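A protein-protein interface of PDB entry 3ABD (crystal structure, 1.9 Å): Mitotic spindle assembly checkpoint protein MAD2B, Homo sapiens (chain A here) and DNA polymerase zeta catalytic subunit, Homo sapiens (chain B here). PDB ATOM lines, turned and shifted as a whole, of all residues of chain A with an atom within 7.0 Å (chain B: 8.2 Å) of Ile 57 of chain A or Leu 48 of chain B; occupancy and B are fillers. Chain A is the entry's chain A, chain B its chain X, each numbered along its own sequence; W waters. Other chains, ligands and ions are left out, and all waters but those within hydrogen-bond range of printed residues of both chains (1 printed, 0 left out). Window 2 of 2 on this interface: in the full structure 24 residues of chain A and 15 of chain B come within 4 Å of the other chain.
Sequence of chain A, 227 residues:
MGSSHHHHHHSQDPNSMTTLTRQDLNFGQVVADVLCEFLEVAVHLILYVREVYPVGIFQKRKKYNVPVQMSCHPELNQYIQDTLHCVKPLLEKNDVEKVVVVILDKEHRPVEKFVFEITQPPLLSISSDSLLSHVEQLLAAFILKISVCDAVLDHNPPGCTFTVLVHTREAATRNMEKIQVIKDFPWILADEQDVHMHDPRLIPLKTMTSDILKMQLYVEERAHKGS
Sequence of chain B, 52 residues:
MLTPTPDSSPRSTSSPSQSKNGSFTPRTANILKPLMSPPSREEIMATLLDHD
OH of Tyr 53 of chain A is in hydrogen-bond range of O of Pro 39 of chain B.
The backbone carbonyl oxygen (O) of Ile 57 of chain A lies within hydrogen-bond range of the backbone NH (N) of Cys 72 of chain A, at 2.7 Å.
N of His 73 of chain A lies within hydrogen-bond range of OG of Ser 71 of chain A (3.1 Å).
A ring nitrogen (ND1) of His 73 of chain A sits at hydrogen-bond distance from the backbone NH (N) of Leu 76 of chain A (3.5 Å).
The side-chain amide oxygen (OD1) of Asn 77 of chain A sits close to the backbone carbonyl oxygen (O) of His 73 of chain A, at 3.2 Å.
OG1 of Thr 47 of chain B sits at hydrogen-bond distance from O of Ile 44 of chain B.
Among the printed residues, merely in contact across the chains: Tyr 53 of chain A with Arg 41 of chain B, Tyr 53 of chain A with Ile 44 of chain B, Pro 54 of chain A with Arg 41 of chain B, Pro 54 of chain A with Met 45 of chain B, Ile 57 of chain A with Ile 44 of chain B, Ile 57 of chain A with Leu 48 of chain B, His 73 of chain A with Ile 44 of chain B and Leu 76 of chain A with Pro 39 of chain B.
No residue of chain B comes within 4 Å of Gly 56 of chain A.
Of chain B, only Ile 44 (3.98 Å) and Leu 48 (3.97 Å) come within 4 Å of Ile 57 of chain A.
Gln 59 of chain A touches none of the printed residues of chain B.
Of the printed residues of chain A, Arg 41 of chain B touches Tyr 53 and Pro 54.
Printed residues of chain A within 4 Å of Ile 44 of chain B: Tyr 53, Ile 57 and His 73.
Printed residues of chain A within 4 Å of Leu 48 of chain B: Ile 57.
The nearest residue of chain B that does not touch Ile 57 of chain A is Met 45 of chain B (6.6 Å).
Of the 14 printed residues of chain A, 5 touch a printed residue of chain B.
Printed residues of chain A that touch a printed residue of chain B: Tyr 53, Pro 54, Ile 57, His 73 and Leu 76.
Of the 9 printed residues of chain B, 5 touch a printed residue of chain A.
Printed residues of chain B that touch a printed residue of chain A: Pro 39, Arg 41, Ile 44, Met 45 and Leu 48.
Among the printed residues, 9 pairs touch across the chains.
Water W1 lies within hydrogen-bond range of a ring nitrogen (NE2) of His 73 of chain A and the backbone carbonyl oxygen (O) of Glu 43 of chain B.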
ATOM      1  N   TYR A  53      17.348 -13.483 -32.292  1.00  0.00           N
ATOM      2  CA  TYR A  53      17.545 -12.069 -32.024  1.00  0.00           C
ATOM      3  C   TYR A  53      18.867 -11.627 -32.583  1.00  0.00           C
ATOM      4  O   TYR A  53      19.720 -12.441 -32.860  1.00  0.00           O
ATOM      5  CB  TYR A  53      17.455 -11.749 -30.526  1.00  0.00           C
ATOM      6  CG  TYR A  53      16.036 -11.986 -30.022  1.00  0.00           C
ATOM      7  CD1 TYR A  53      15.069 -11.008 -30.122  1.00  0.00           C
ATOM      8  CD2 TYR A  53      15.656 -13.214 -29.503  1.00  0.00           C
ATOM      9  CE1 TYR A  53      13.780 -11.238 -29.699  1.00  0.00           C
ATOM     10  CE2 TYR A  53      14.354 -13.439 -29.077  1.00  0.00           C
ATOM     11  CZ  TYR A  53      13.443 -12.485 -29.151  1.00  0.00           C
ATOM     12  OH  TYR A  53      12.144 -12.693 -28.710  1.00  0.00           O
ATOM     13  N   PRO A  54      18.997 -10.313 -32.823  1.00  0.00           N
ATOM     14  CA  PRO A  54      20.237  -9.792 -33.415  1.00  0.00           C
ATOM     15  C   PRO A  54      21.425 -10.075 -32.519  1.00  0.00           C
ATOM     16  O   PRO A  54      21.320  -9.905 -31.324  1.00  0.00           O
ATOM     17  CB  PRO A  54      20.028  -8.300 -33.465  1.00  0.00           C
ATOM     18  CG  PRO A  54      18.610  -8.020 -32.987  1.00  0.00           C
ATOM     19  CD  PRO A  54      18.058  -9.260 -32.363  1.00  0.00           C
ATOM     20  N   VAL A  55      22.613 -10.402 -33.097  1.00  0.00           N
ATOM     21  CA  VAL A  55      23.833 -10.659 -32.319  1.00  0.00           C
ATOM     22  C   VAL A  55      24.211  -9.479 -31.383  1.00  0.00           C
ATOM     23  O   VAL A  55      24.765  -9.689 -30.306  1.00  0.00           O
ATOM     24  CB  VAL A  55      25.034 -10.953 -33.247  1.00  0.00           C
ATOM     25  CG1 VAL A  55      24.806 -12.240 -34.029  1.00  0.00           C
ATOM     26  CG2 VAL A  55      25.278  -9.784 -34.186  1.00  0.00           C
ATOM     27  N   GLY A  56      23.845  -8.287 -31.799  1.00  0.00           N
ATOM     28  CA  GLY A  56      24.150  -7.093 -31.039  1.00  0.00           C
ATOM     29  C   GLY A  56      23.632  -7.041 -29.607  1.00  0.00           C
ATOM     30  O   GLY A  56      24.215  -6.327 -28.796  1.00  0.00           O
ATOM     31  N   ILE A  57      22.557  -7.780 -29.286  1.00  0.00           N
ATOM     32  CA  ILE A  57      21.987  -7.735 -27.928  1.00  0.00           C
ATOM     33  C   ILE A  57      22.637  -8.709 -26.994  1.00  0.00           C
ATOM     34  O   ILE A  57      22.406  -8.635 -25.796  1.00  0.00           O
ATOM     35  CB  ILE A  57      20.444  -7.887 -27.833  1.00  0.00           C
ATOM     36  CG1 ILE A  57      19.973  -9.300 -28.203  1.00  0.00           C
ATOM     37  CG2 ILE A  57      19.788  -6.877 -28.703  1.00  0.00           C
ATOM     38  CD1 ILE A  57      18.571  -9.660 -27.675  1.00  0.00           C
ATOM     39  N   PHE A  58      23.520  -9.563 -27.520  1.00  0.00           N
ATOM     40  CA  PHE A  58      24.171 -10.620 -26.722  1.00  0.00           C
ATOM     41  C   PHE A  58      25.585 -10.260 -26.379  1.00  0.00           C
ATOM     42  O   PHE A  58      26.290  -9.620 -27.150  1.00  0.00           O
ATOM     43  CB  PHE A  58      24.213 -11.960 -27.460  1.00  0.00           C
ATOM     44  CG  PHE A  58      22.877 -12.546 -27.695  1.00  0.00           C
ATOM     45  CD1 PHE A  58      22.301 -13.386 -26.788  1.00  0.00           C
ATOM     46  CD2 PHE A  58      22.201 -12.267 -28.852  1.00  0.00           C
ATOM     47  CE1 PHE A  58      21.001 -13.953 -27.078  1.00  0.00           C
ATOM     48  CE2 PHE A  58      20.946 -12.807 -29.144  1.00  0.00           C
ATOM     49  CZ  PHE A  58      20.363 -13.629 -28.262  1.00  0.00           C
ATOM     50  N   GLN A  59      25.996 -10.619 -25.136  1.00  0.00           N
ATOM     51  CA  GLN A  59      27.291 -10.417 -24.563  1.00  0.00           C
ATOM     52  C   GLN A  59      27.876 -11.749 -24.181  1.00  0.00           C
ATOM     53  O   GLN A  59      27.162 -12.579 -23.661  1.00  0.00           O
ATOM     54  CB  GLN A  59      27.133  -9.605 -23.286  1.00  0.00           C
ATOM     55  CG  GLN A  59      28.388  -9.227 -22.654  1.00  0.00           C
ATOM     56  CD  GLN A  59      28.158  -8.305 -21.478  1.00  0.00           C
ATOM     57  OE1 GLN A  59      27.049  -7.915 -21.215  1.00  0.00           O
ATOM     58  NE2 GLN A  59      29.209  -7.972 -20.783  1.00  0.00           N
ATOM     59  N   GLN A  69      26.707 -16.924 -24.522  1.00  0.00           N
ATOM     60  CA  GLN A  69      26.213 -15.605 -24.968  1.00  0.00           C
ATOM     61  C   GLN A  69      24.850 -15.336 -24.265  1.00  0.00           C
ATOM     62  O   GLN A  69      23.944 -16.202 -24.280  1.00  0.00           O
ATOM     63  CB  GLN A  69      26.075 -15.603 -26.475  1.00  0.00           C
ATOM     64  CG  GLN A  69      27.401 -15.638 -27.234  1.00  0.00           C
ATOM     65  CD  GLN A  69      28.073 -14.279 -27.355  1.00  0.00           C
ATOM     66  OE1 GLN A  69      27.390 -13.252 -27.429  1.00  0.00           O
ATOM     67  NE2 GLN A  69      29.414 -14.270 -27.461  1.00  0.00           N
ATOM     68  N   MET A  70      24.745 -14.181 -23.602  1.00  0.00           N
ATOM     69  CA  MET A  70      23.553 -13.824 -22.827  1.00  0.00           C
ATOM     70  C   MET A  70      23.005 -12.520 -23.396  1.00  0.00           C
ATOM     71  O   MET A  70      23.767 -11.543 -23.588  1.00  0.00           O
ATOM     72  CB  MET A  70      23.808 -13.608 -21.328  1.00  0.00           C
ATOM     73  CG  MET A  70      24.340 -14.812 -20.366  1.00  0.00           C
ATOM     74  SD  MET A  70      23.176 -16.136 -20.278  1.00  0.00           S
ATOM     75  CE  MET A  70      21.891 -15.605 -19.165  1.00  0.00           C
ATOM     76  N   SER A  71      21.697 -12.471 -23.608  1.00  0.00           N
ATOM     77  CA  SER A  71      21.042 -11.226 -23.992  1.00  0.00           C
ATOM     78  C   SER A  71      21.179 -10.124 -22.872  1.00  0.00           C
ATOM     79  O   SER A  71      21.075 -10.399 -21.679  1.00  0.00           O
ATOM     80  CB  SER A  71      19.569 -11.522 -24.292  1.00  0.00           C
ATOM     81  OG  SER A  71      18.724 -10.411 -24.095  1.00  0.00           O
ATOM     82  N   CYS A  72      21.423  -8.910 -23.281  1.00  0.00           N
ATOM     83  CA  CYS A  72      21.469  -7.744 -22.401  1.00  0.00           C
ATOM     84  C   CYS A  72      20.129  -6.952 -22.512  1.00  0.00           C
ATOM     85  O   CYS A  72      19.974  -5.888 -21.935  1.00  0.00           O
ATOM     86  CB  CYS A  72      22.655  -6.879 -22.843  1.00  0.00           C
ATOM     87  SG  CYS A  72      24.130  -7.730 -22.377  1.00  0.00           S
ATOM     88  N   HIS A  73      19.182  -7.431 -23.301  1.00  0.00           N
ATOM     89  CA  HIS A  73      17.920  -6.702 -23.445  1.00  0.00           C
ATOM     90  C   HIS A  73      16.914  -7.049 -22.299  1.00  0.00           C
ATOM     91  O   HIS A  73      16.494  -8.224 -22.148  1.00  0.00           O
ATOM     92  CB  HIS A  73      17.299  -6.944 -24.815  1.00  0.00           C
ATOM     93  CG  HIS A  73      16.134  -6.065 -25.089  1.00  0.00           C
ATOM     94  ND1 HIS A  73      14.878  -6.326 -24.592  1.00  0.00           N
ATOM     95  CD2 HIS A  73      16.038  -4.900 -25.769  1.00  0.00           C
ATOM     96  CE1 HIS A  73      14.069  -5.335 -24.921  1.00  0.00           C
ATOM     97  NE2 HIS A  73      14.745  -4.469 -25.652  1.00  0.00           N
ATOM     98  N   LEU A  76      13.364  -9.021 -23.023  1.00  0.00           N
ATOM     99  CA  LEU A  76      13.583 -10.393 -23.368  1.00  0.00           C
ATOM    100  C   LEU A  76      13.956 -11.187 -22.088  1.00  0.00           C
ATOM    101  O   LEU A  76      13.428 -12.262 -21.855  1.00  0.00           O
ATOM    102  CB  LEU A  76      14.667 -10.506 -24.454  1.00  0.00           C
ATOM    103  CG  LEU A  76      15.034 -11.904 -24.921  1.00  0.00           C
ATOM    104  CD1 LEU A  76      13.772 -12.707 -25.320  1.00  0.00           C
ATOM    105  CD2 LEU A  76      16.056 -11.886 -26.116  1.00  0.00           C
ATOM    106  N   ASN A  77      14.875 -10.642 -21.285  1.00  0.00           N
ATOM    107  CA  ASN A  77      15.446 -11.352 -20.193  1.00  0.00           C
ATOM    108  C   ASN A  77      14.361 -11.580 -19.182  1.00  0.00           C
ATOM    109  O   ASN A  77      14.291 -12.640 -18.544  1.00  0.00           O
ATOM    110  CB  ASN A  77      16.653 -10.635 -19.535  1.00  0.00           C
ATOM    111  CG  ASN A  77      17.846 -10.470 -20.481  1.00  0.00           C
ATOM    112  OD1 ASN A  77      17.890 -11.076 -21.565  1.00  0.00           O
ATOM    113  ND2 ASN A  77      18.822  -9.638 -20.070  1.00  0.00           N
ATOM    114  N   PRO B  39       9.117 -10.479 -26.696  1.00  0.00           N
ATOM    115  CA  PRO B  39       9.135  -9.303 -27.609  1.00  0.00           C
ATOM    116  C   PRO B  39       9.589  -9.694 -29.024  1.00  0.00           C
ATOM    117  O   PRO B  39      10.467 -10.519 -29.171  1.00  0.00           O
ATOM    118  CB  PRO B  39      10.118  -8.347 -26.940  1.00  0.00           C
ATOM    119  CG  PRO B  39      10.783  -9.102 -25.851  1.00  0.00           C
ATOM    120  CD  PRO B  39       9.940 -10.277 -25.499  1.00  0.00           C
ATOM    121  N   ARG B  41      11.637  -9.493 -32.492  1.00  0.00           N
ATOM    122  CA  ARG B  41      12.911  -8.982 -32.936  1.00  0.00           C
ATOM    123  C   ARG B  41      12.719  -7.569 -33.505  1.00  0.00           C
ATOM    124  O   ARG B  41      13.556  -6.696 -33.297  1.00  0.00           O
ATOM    125  CB  ARG B  41      13.454  -9.924 -33.996  1.00  0.00           C
ATOM    126  CG  ARG B  41      14.831  -9.617 -34.538  1.00  0.00           C
ATOM    127  CD  ARG B  41      15.118 -10.499 -35.737  1.00  0.00           C
ATOM    128  NE  ARG B  41      16.391 -10.186 -36.380  1.00  0.00           N
ATOM    129  CZ  ARG B  41      17.468 -10.975 -36.327  1.00  0.00           C
ATOM    130  NH1 ARG B  41      17.439 -12.118 -35.659  1.00  0.00           N
ATOM    131  NH2 ARG B  41      18.586 -10.619 -36.927  1.00  0.00           N
ATOM    132  N   GLU B  42      11.530  -7.401 -34.161  1.00  0.00           N
ATOM    133  CA  GLU B  42      11.322  -6.084 -34.728  1.00  0.00           C
ATOM    134  C   GLU B  42      11.211  -5.081 -33.589  1.00  0.00           C
ATOM    135  O   GLU B  42      11.729  -3.958 -33.683  1.00  0.00           O
ATOM    136  CB  GLU B  42      10.086  -6.030 -35.660  1.00  0.00           C
ATOM    137  CG  GLU B  42      10.198  -6.864 -36.919  1.00  0.00           C
ATOM    138  CD  GLU B  42       9.774  -8.314 -36.725  1.00  0.00           C
ATOM    139  OE1 GLU B  42       9.480  -8.696 -35.570  1.00  0.00           O
ATOM    140  OE2 GLU B  42       9.719  -9.068 -37.738  1.00  0.00           O
ATOM    141  N   GLU B  43      10.461  -5.456 -32.575  1.00  0.00           N
ATOM    142  CA  GLU B  43      10.243  -4.586 -31.463  1.00  0.00           C
ATOM    143  C   GLU B  43      11.605  -4.248 -30.874  1.00  0.00           C
ATOM    144  O   GLU B  43      11.847  -3.126 -30.528  1.00  0.00           O
ATOM    145  CB  GLU B  43       9.385  -5.265 -30.393  1.00  0.00           C
ATOM    146  CG  GLU B  43       7.908  -5.430 -30.649  1.00  0.00           C
ATOM    147  CD  GLU B  43       7.294  -6.430 -29.666  1.00  0.00           C
ATOM    148  OE1 GLU B  43       7.460  -6.273 -28.439  1.00  0.00           O
ATOM    149  OE2 GLU B  43       6.699  -7.398 -30.122  1.00  0.00           O
ATOM    150  N   ILE B  44      12.489  -5.228 -30.762  1.00  0.00           N
ATOM    151  CA  ILE B  44      13.816  -4.977 -30.178  1.00  0.00           C
ATOM    152  C   ILE B  44      14.569  -3.993 -31.089  1.00  0.00           C
ATOM    153  O   ILE B  44      15.133  -2.988 -30.637  1.00  0.00           O
ATOM    154  CB  ILE B  44      14.661  -6.244 -30.051  1.00  0.00           C
ATOM    155  CG1 ILE B  44      13.918  -7.396 -29.338  1.00  0.00           C
ATOM    156  CG2 ILE B  44      15.992  -5.900 -29.382  1.00  0.00           C
ATOM    157  CD1 ILE B  44      13.979  -7.391 -27.890  1.00  0.00           C
ATOM    158  N   MET B  45      14.549  -4.266 -32.385  1.00  0.00           N
ATOM    159  CA  MET B  45      15.299  -3.459 -33.326  1.00  0.00           C
ATOM    160  C   MET B  45      14.871  -2.001 -33.273  1.00  0.00           C
ATOM    161  O   MET B  45      15.704  -1.118 -33.405  1.00  0.00           O
ATOM    162  CB  MET B  45      15.179  -4.023 -34.745  1.00  0.00           C
ATOM    163  CG  MET B  45      15.978  -5.302 -34.939  1.00  0.00           C
ATOM    164  SD  MET B  45      17.756  -5.019 -34.715  1.00  0.00           S
ATOM    165  CE  MET B  45      18.110  -3.783 -35.968  1.00  0.00           C
ATOM    166  N   ALA B  46      13.593  -1.769 -33.020  1.00  0.00           N
ATOM    167  CA  ALA B  46      13.032  -0.420 -32.879  1.00  0.00           C
ATOM    168  C   ALA B  46      13.712   0.429 -31.793  1.00  0.00           C
ATOM    169  O   ALA B  46      13.707   1.655 -31.878  1.00  0.00           O
ATOM    170  CB  ALA B  46      11.545  -0.516 -32.548  1.00  0.00           C
ATOM    171  N   THR B  47      14.232  -0.228 -30.760  1.00  0.00           N
ATOM    172  CA  THR B  47      14.835   0.451 -29.601  1.00  0.00           C
ATOM    173  C   THR B  47      16.326   0.706 -29.794  1.00  0.00           C
ATOM    174  O   THR B  47      16.895   1.523 -29.085  1.00  0.00           O
ATOM    175  CB  THR B  47      14.640  -0.361 -28.323  1.00  0.00           C
ATOM    176  OG1 THR B  47      15.386  -1.578 -28.407  1.00  0.00           O
ATOM    177  CG2 THR B  47      13.160  -0.698 -28.109  1.00  0.00           C
ATOM    178  N   LEU B  48      16.921   0.037 -30.784  1.00  0.00           N
ATOM    179  CA  LEU B  48      18.362   0.030 -31.033  1.00  0.00           C
ATOM    180  C   LEU B  48      18.771   1.070 -32.078  1.00  0.00           C
ATOM    181  O   LEU B  48      17.946   1.412 -32.925  1.00  0.00           O
ATOM    182  CB  LEU B  48      18.810  -1.351 -31.525  1.00  0.00           C
ATOM    183  CG  LEU B  48      19.265  -2.404 -30.510  1.00  0.00           C
ATOM    184  CD1 LEU B  48      18.431  -2.388 -29.267  1.00  0.00           C
ATOM    185  CD2 LEU B  48      19.284  -3.774 -31.128  1.00  0.00           C
HETATM  186  O   HOH W   1      11.826  -3.348 -27.055  1.00  0.00           O
